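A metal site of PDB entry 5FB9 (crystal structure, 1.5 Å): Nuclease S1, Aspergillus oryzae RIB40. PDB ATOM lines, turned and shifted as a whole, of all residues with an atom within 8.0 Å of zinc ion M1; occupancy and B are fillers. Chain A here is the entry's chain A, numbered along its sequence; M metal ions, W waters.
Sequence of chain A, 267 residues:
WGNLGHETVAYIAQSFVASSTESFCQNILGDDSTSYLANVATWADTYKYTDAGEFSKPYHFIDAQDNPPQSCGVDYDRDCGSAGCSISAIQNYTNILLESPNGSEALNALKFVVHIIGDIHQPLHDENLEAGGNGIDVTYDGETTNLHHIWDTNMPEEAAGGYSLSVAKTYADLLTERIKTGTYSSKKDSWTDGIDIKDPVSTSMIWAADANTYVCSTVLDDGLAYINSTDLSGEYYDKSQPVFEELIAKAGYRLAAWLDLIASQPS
Within 4 Å of zinc ion M1: His 125, His 148 and Asp 152.
The backbone NH (N) of Trp 1 sits close to the side-chain carboxylate (OD1) of Asp 152 (3.0 Å). The side-chain carboxylate (OD1) of Asp 152 lies within hydrogen-bond range of the side-chain amide nitrogen (NE2) of Gln 122. O of Asp 152 lies within hydrogen-bond range of N of Gly 2, 2.9 Å away. O of Gly 132 sits at hydrogen-bond distance from ND1 of His 148, 2.8 Å away. The backbone NH (N) of His 148 is in hydrogen-bond range of the side-chain amide oxygen (OD1) of Asn 146 (3.1 Å). A ring nitrogen (ND1) of His 125 sits at hydrogen-bond distance from the backbone carbonyl oxygen (O) of His 60 (2.7 Å).
Zinc ion M1 is bound by the side-chain carboxylate of Asp 152 (2.0 Å), water W1 (2.0 Å), water W2 (2.1 Å), a ring nitrogen (NE2) of His 148 (2.1 Å) and a ring nitrogen (NE2) of His 125 (2.1 Å). Slightly farther from zinc ion M1 lies the side-chain carboxylate (OD1) of Asp 152 (2.7 Å).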
ATOM      1  N   TRP A   1     -10.532  -8.835   2.915  1.00  0.00           N
ATOM      2  CA  TRP A   1     -10.592  -7.327   2.735  1.00  0.00           C
ATOM      3  C   TRP A   1     -11.849  -7.002   1.987  1.00  0.00           C
ATOM      4  O   TRP A   1     -12.409  -7.815   1.277  1.00  0.00           O
ATOM      5  CB  TRP A   1      -9.400  -6.772   1.910  1.00  0.00           C
ATOM      6  CG  TRP A   1      -8.051  -7.240   2.360  1.00  0.00           C
ATOM      7  CD1 TRP A   1      -7.340  -8.258   1.818  1.00  0.00           C
ATOM      8  CD2 TRP A   1      -7.274  -6.758   3.436  1.00  0.00           C
ATOM      9  NE1 TRP A   1      -6.168  -8.417   2.447  1.00  0.00           N
ATOM     10  CE2 TRP A   1      -6.074  -7.502   3.466  1.00  0.00           C
ATOM     11  CE3 TRP A   1      -7.456  -5.765   4.394  1.00  0.00           C
ATOM     12  CZ2 TRP A   1      -5.090  -7.298   4.422  1.00  0.00           C
ATOM     13  CZ3 TRP A   1      -6.480  -5.542   5.305  1.00  0.00           C
ATOM     14  CH2 TRP A   1      -5.309  -6.314   5.340  1.00  0.00           C
ATOM     15  N   GLY A   2     -12.209  -5.733   2.077  1.00  0.00           N
ATOM     16  CA  GLY A   2     -13.221  -5.145   1.190  1.00  0.00           C
ATOM     17  C   GLY A   2     -12.639  -4.840  -0.188  1.00  0.00           C
ATOM     18  O   GLY A   2     -11.462  -5.166  -0.479  1.00  0.00           O
ATOM     19  N   HIS A   6      -8.669  -5.474  -1.897  1.00  0.00           N
ATOM     20  CA  HIS A   6      -8.442  -6.384  -3.028  1.00  0.00           C
ATOM     21  C   HIS A   6      -7.882  -5.726  -4.290  1.00  0.00           C
ATOM     22  O   HIS A   6      -7.004  -6.264  -4.957  1.00  0.00           O
ATOM     23  CB  HIS A   6      -9.695  -7.190  -3.346  1.00  0.00           C
ATOM     24  CG  HIS A   6      -9.969  -8.202  -2.310  1.00  0.00           C
ATOM     25  ND1 HIS A   6      -9.180  -9.318  -2.181  1.00  0.00           N
ATOM     26  CD2 HIS A   6     -10.805  -8.226  -1.244  1.00  0.00           C
ATOM     27  CE1 HIS A   6      -9.544 -10.017  -1.128  1.00  0.00           C
ATOM     28  NE2 HIS A   6     -10.518  -9.358  -0.507  1.00  0.00           N
ATOM     29  N   ASP A  45     -16.119 -11.798  -4.120  1.00  0.00           N
ATOM     30  CA  ASP A  45     -16.970 -11.265  -3.071  1.00  0.00           C
ATOM     31  C   ASP A  45     -18.390 -10.981  -3.542  1.00  0.00           C
ATOM     32  O   ASP A  45     -19.256 -10.772  -2.680  1.00  0.00           O
ATOM     33  CB  ASP A  45     -16.350  -9.998  -2.398  1.00  0.00           C
ATOM     34  CG  ASP A  45     -15.366 -10.339  -1.262  1.00  0.00           C
ATOM     35  OD1 ASP A  45     -15.283 -11.533  -0.870  1.00  0.00           O
ATOM     36  OD2 ASP A  45     -14.687  -9.425  -0.773  1.00  0.00           O
ATOM     37  N   LYS A  48     -20.041 -14.963  -4.206  1.00  0.00           N
ATOM     38  CA  LYS A  48     -20.403 -15.741  -3.027  1.00  0.00           C
ATOM     39  C   LYS A  48     -21.836 -15.520  -2.534  1.00  0.00           C
ATOM     40  O   LYS A  48     -22.307 -16.282  -1.730  1.00  0.00           O
ATOM     41  CB  LYS A  48     -19.405 -15.515  -1.898  1.00  0.00           C
ATOM     42  CG  LYS A  48     -19.504 -14.158  -1.240  1.00  0.00           C
ATOM     43  CD  LYS A  48     -18.335 -13.916  -0.280  1.00  0.00           C
ATOM     44  CE  LYS A  48     -18.386 -12.562   0.393  1.00  0.00           C
ATOM     45  NZ  LYS A  48     -17.165 -12.297   1.217  1.00  0.00           N
ATOM     46  N   HIS A  60     -12.692 -17.917   1.455  1.00  0.00           N
ATOM     47  CA  HIS A  60     -12.065 -16.660   1.809  1.00  0.00           C
ATOM     48  C   HIS A  60     -11.271 -16.744   3.115  1.00  0.00           C
ATOM     49  O   HIS A  60     -10.576 -15.771   3.479  1.00  0.00           O
ATOM     50  CB  HIS A  60     -13.182 -15.608   1.897  1.00  0.00           C
ATOM     51  CG  HIS A  60     -13.887 -15.393   0.609  1.00  0.00           C
ATOM     52  ND1 HIS A  60     -13.873 -14.198  -0.056  1.00  0.00           N
ATOM     53  CD2 HIS A  60     -14.551 -16.259  -0.178  1.00  0.00           C
ATOM     54  CE1 HIS A  60     -14.517 -14.335  -1.208  1.00  0.00           C
ATOM     55  NE2 HIS A  60     -14.936 -15.578  -1.304  1.00  0.00           N
ATOM     56  N   PHE A  61     -11.362 -17.874   3.793  1.00  0.00           N
ATOM     57  CA  PHE A  61     -10.915 -18.017   5.180  1.00  0.00           C
ATOM     58  C   PHE A  61     -10.135 -19.283   5.418  1.00  0.00           C
ATOM     59  O   PHE A  61     -10.411 -20.292   4.764  1.00  0.00           O
ATOM     60  CB  PHE A  61     -12.136 -18.107   6.162  1.00  0.00           C
ATOM     61  CG  PHE A  61     -13.205 -17.043   5.967  1.00  0.00           C
ATOM     62  CD1 PHE A  61     -12.935 -15.722   6.344  1.00  0.00           C
ATOM     63  CD2 PHE A  61     -14.418 -17.336   5.426  1.00  0.00           C
ATOM     64  CE1 PHE A  61     -13.898 -14.732   6.188  1.00  0.00           C
ATOM     65  CE2 PHE A  61     -15.392 -16.366   5.240  1.00  0.00           C
ATOM     66  CZ  PHE A  61     -15.131 -15.053   5.633  1.00  0.00           C
ATOM     67  N   HIS A 115      -8.064 -12.856  -5.813  1.00  0.00           N
ATOM     68  CA  HIS A 115      -8.790 -12.468  -4.586  1.00  0.00           C
ATOM     69  C   HIS A 115      -8.259 -13.112  -3.340  1.00  0.00           C
ATOM     70  O   HIS A 115      -8.034 -12.462  -2.316  1.00  0.00           O
ATOM     71  CB  HIS A 115     -10.291 -12.810  -4.764  1.00  0.00           C
ATOM     72  CG  HIS A 115     -11.160 -12.348  -3.635  1.00  0.00           C
ATOM     73  ND1 HIS A 115     -11.706 -11.081  -3.581  1.00  0.00           N
ATOM     74  CD2 HIS A 115     -11.535 -12.974  -2.500  1.00  0.00           C
ATOM     75  CE1 HIS A 115     -12.406 -10.975  -2.456  1.00  0.00           C
ATOM     76  NE2 HIS A 115     -12.268 -12.073  -1.752  1.00  0.00           N
ATOM     77  N   ASP A 119      -7.068 -12.240   0.545  1.00  0.00           N
ATOM     78  CA  ASP A 119      -7.684 -12.620   1.814  1.00  0.00           C
ATOM     79  C   ASP A 119      -6.775 -13.350   2.796  1.00  0.00           C
ATOM     80  O   ASP A 119      -6.840 -13.120   3.980  1.00  0.00           O
ATOM     81  CB  ASP A 119      -8.936 -13.440   1.578  1.00  0.00           C
ATOM     82  CG  ASP A 119     -10.135 -12.598   1.332  1.00  0.00           C
ATOM     83  OD1 ASP A 119     -10.152 -11.396   1.618  1.00  0.00           O
ATOM     84  OD2 ASP A 119     -11.124 -13.174   0.831  1.00  0.00           O
ATOM     85  N   GLN A 122      -5.202 -10.986   5.218  1.00  0.00           N
ATOM     86  CA  GLN A 122      -6.018 -10.258   6.209  1.00  0.00           C
ATOM     87  C   GLN A 122      -5.986 -11.129   7.436  1.00  0.00           C
ATOM     88  O   GLN A 122      -6.559 -12.234   7.369  1.00  0.00           O
ATOM     89  CB  GLN A 122      -7.429 -10.001   5.628  1.00  0.00           C
ATOM     90  CG  GLN A 122      -8.193  -8.799   6.168  1.00  0.00           C
ATOM     91  CD  GLN A 122      -8.662  -8.917   7.595  1.00  0.00           C
ATOM     92  OE1 GLN A 122      -7.861  -9.189   8.491  1.00  0.00           O
ATOM     93  NE2 GLN A 122      -9.959  -8.697   7.850  1.00  0.00           N
ATOM     94  N   LEU A 124      -7.526 -11.488  10.237  1.00  0.00           N
ATOM     95  CA  LEU A 124      -8.813 -12.025  10.683  1.00  0.00           C
ATOM     96  C   LEU A 124      -9.548 -12.861   9.693  1.00  0.00           C
ATOM     97  O   LEU A 124     -10.610 -13.386  10.038  1.00  0.00           O
ATOM     98  CB  LEU A 124      -9.712 -10.901  11.243  1.00  0.00           C
ATOM     99  CG  LEU A 124      -9.238 -10.302  12.581  1.00  0.00           C
ATOM    100  CD1 LEU A 124     -10.087  -9.110  12.976  1.00  0.00           C
ATOM    101  CD2 LEU A 124      -9.212 -11.360  13.683  1.00  0.00           C
ATOM    102  N   HIS A 125      -9.031 -13.028   8.467  1.00  0.00           N
ATOM    103  CA  HIS A 125      -9.403 -14.111   7.565  1.00  0.00           C
ATOM    104  C   HIS A 125      -8.696 -15.431   7.884  1.00  0.00           C
ATOM    105  O   HIS A 125      -8.999 -16.455   7.257  1.00  0.00           O
ATOM    106  CB  HIS A 125      -9.190 -13.720   6.113  1.00  0.00           C
ATOM    107  CG  HIS A 125     -10.305 -12.911   5.545  1.00  0.00           C
ATOM    108  ND1 HIS A 125     -11.060 -13.332   4.486  1.00  0.00           N
ATOM    109  CD2 HIS A 125     -10.816 -11.722   5.924  1.00  0.00           C
ATOM    110  CE1 HIS A 125     -12.042 -12.460   4.270  1.00  0.00           C
ATOM    111  NE2 HIS A 125     -11.884 -11.465   5.101  1.00  0.00           N
ATOM    112  N   ALA A 131     -15.949 -15.938  14.796  1.00  0.00           N
ATOM    113  CA  ALA A 131     -16.097 -15.915  13.348  1.00  0.00           C
ATOM    114  C   ALA A 131     -15.133 -14.882  12.759  1.00  0.00           C
ATOM    115  O   ALA A 131     -15.539 -13.947  12.066  1.00  0.00           O
ATOM    116  CB  ALA A 131     -17.533 -15.671  12.961  1.00  0.00           C
ATOM    117  N   GLY A 132     -13.848 -15.028  13.068  1.00  0.00           N
ATOM    118  CA  GLY A 132     -12.854 -14.100  12.569  1.00  0.00           C
ATOM    119  C   GLY A 132     -13.068 -12.685  13.050  1.00  0.00           C
ATOM    120  O   GLY A 132     -12.772 -11.743  12.322  1.00  0.00           O
ATOM    121  N   ASN A 134     -15.888 -11.191  13.595  1.00  0.00           N
ATOM    122  CA  ASN A 134     -17.219 -10.682  13.254  1.00  0.00           C
ATOM    123  C   ASN A 134     -18.087 -10.533  14.516  1.00  0.00           C
ATOM    124  O   ASN A 134     -18.863  -9.567  14.624  1.00  0.00           O
ATOM    125  CB  ASN A 134     -17.929 -11.470  12.163  1.00  0.00           C
ATOM    126  CG  ASN A 134     -17.410 -11.129  10.765  1.00  0.00           C
ATOM    127  OD1 ASN A 134     -17.574 -10.017  10.244  1.00  0.00           O
ATOM    128  ND2 ASN A 134     -16.824 -12.103  10.146  1.00  0.00           N
ATOM    129  N   ASN A 146     -17.781  -3.990  13.781  1.00  0.00           N
ATOM    130  CA  ASN A 146     -17.116  -5.120  14.426  1.00  0.00           C
ATOM    131  C   ASN A 146     -15.660  -5.188  14.038  1.00  0.00           C
ATOM    132  O   ASN A 146     -15.227  -4.526  13.083  1.00  0.00           O
ATOM    133  CB  ASN A 146     -17.893  -6.407  14.132  1.00  0.00           C
ATOM    134  CG  ASN A 146     -17.822  -6.801  12.678  1.00  0.00           C
ATOM    135  OD1 ASN A 146     -16.745  -7.201  12.187  1.00  0.00           O
ATOM    136  ND2 ASN A 146     -18.933  -6.780  12.002  1.00  0.00           N
ATOM    137  N   HIS A 148     -13.712  -7.520  12.698  1.00  0.00           N
ATOM    138  CA  HIS A 148     -13.420  -7.981  11.366  1.00  0.00           C
ATOM    139  C   HIS A 148     -13.588  -6.878  10.329  1.00  0.00           C
ATOM    140  O   HIS A 148     -12.702  -6.670   9.476  1.00  0.00           O
ATOM    141  CB  HIS A 148     -14.323  -9.196  11.009  1.00  0.00           C
ATOM    142  CG  HIS A 148     -13.935  -9.864   9.743  1.00  0.00           C
ATOM    143  ND1 HIS A 148     -13.181 -11.022   9.689  1.00  0.00           N
ATOM    144  CD2 HIS A 148     -14.141  -9.488   8.478  1.00  0.00           C
ATOM    145  CE1 HIS A 148     -12.953 -11.317   8.417  1.00  0.00           C
ATOM    146  NE2 HIS A 148     -13.515 -10.406   7.670  1.00  0.00           N
ATOM    147  N   HIS A 149     -14.709  -6.209  10.410  1.00  0.00           N
ATOM    148  CA  HIS A 149     -15.064  -5.173   9.432  1.00  0.00           C
ATOM    149  C   HIS A 149     -14.026  -4.033   9.424  1.00  0.00           C
ATOM    150  O   HIS A 149     -13.731  -3.496   8.374  1.00  0.00           O
ATOM    151  CB  HIS A 149     -16.457  -4.621   9.761  1.00  0.00           C
ATOM    152  CG  HIS A 149     -17.078  -3.792   8.671  1.00  0.00           C
ATOM    153  ND1 HIS A 149     -16.952  -2.432   8.639  1.00  0.00           N
ATOM    154  CD2 HIS A 149     -17.871  -4.132   7.619  1.00  0.00           C
ATOM    155  CE1 HIS A 149     -17.566  -1.965   7.547  1.00  0.00           C
ATOM    156  NE2 HIS A 149     -18.150  -2.971   6.940  1.00  0.00           N
ATOM    157  N   TRP A 151     -10.850  -4.165  10.014  1.00  0.00           N
ATOM    158  CA  TRP A 151      -9.663  -4.657   9.313  1.00  0.00           C
ATOM    159  C   TRP A 151      -9.968  -4.784   7.821  1.00  0.00           C
ATOM    160  O   TRP A 151      -9.079  -4.523   6.997  1.00  0.00           O
ATOM    161  CB  TRP A 151      -9.177  -5.994   9.962  1.00  0.00           C
ATOM    162  CG  TRP A 151      -8.336  -5.717  11.188  1.00  0.00           C
ATOM    163  CD1 TRP A 151      -8.770  -5.481  12.448  1.00  0.00           C
ATOM    164  CD2 TRP A 151      -6.913  -5.553  11.229  1.00  0.00           C
ATOM    165  NE1 TRP A 151      -7.728  -5.179  13.273  1.00  0.00           N
ATOM    166  CE2 TRP A 151      -6.560  -5.204  12.558  1.00  0.00           C
ATOM    167  CE3 TRP A 151      -5.888  -5.704  10.275  1.00  0.00           C
ATOM    168  CZ2 TRP A 151      -5.248  -4.962  12.941  1.00  0.00           C
ATOM    169  CZ3 TRP A 151      -4.599  -5.464  10.657  1.00  0.00           C
ATOM    170  CH2 TRP A 151      -4.272  -5.112  11.971  1.00  0.00           C
ATOM    171  N   ASP A 152     -11.158  -5.222   7.436  1.00  0.00           N
ATOM    172  CA  ASP A 152     -11.466  -5.404   6.042  1.00  0.00           C
ATOM    173  C   ASP A 152     -11.549  -4.052   5.323  1.00  0.00           C
ATOM    174  O   ASP A 152     -11.163  -3.940   4.161  1.00  0.00           O
ATOM    175  CB  ASP A 152     -12.834  -6.119   5.816  1.00  0.00           C
ATOM    176  CG  ASP A 152     -12.741  -7.627   5.737  1.00  0.00           C
ATOM    177  OD1 ASP A 152     -11.669  -8.227   5.637  1.00  0.00           O
ATOM    178  OD2 ASP A 152     -13.832  -8.184   5.782  1.00  0.00           O
ATOM    179  N   THR A 153     -12.122  -3.071   6.004  1.00  0.00           N
ATOM    180  CA  THR A 153     -12.712  -1.928   5.371  1.00  0.00           C
ATOM    181  C   THR A 153     -12.394  -0.577   6.034  1.00  0.00           C
ATOM    182  O   THR A 153     -11.796   0.274   5.402  1.00  0.00           O
ATOM    183  CB  THR A 153     -14.231  -2.147   5.258  1.00  0.00           C
ATOM    184  OG1 THR A 153     -14.480  -3.251   4.356  1.00  0.00           O
ATOM    185  CG2 THR A 153     -14.998  -0.951   4.739  1.00  0.00           C
HETATM  186 ZN    ZN M   1     -13.497 -10.151   5.575  1.00  0.00          ZN
HETATM  187 ZN    ZN M   2     -11.423  -9.753   1.268  1.00  0.00          ZN
HETATM  188 ZN    ZN M   3     -12.951 -12.418   0.155  1.00  0.00          ZN
HETATM  189  O   HOH W   1     -13.745  -9.733   3.620  1.00  0.00           O
HETATM  190  O   HOH W   2     -15.290 -11.240   5.451  1.00  0.00           O
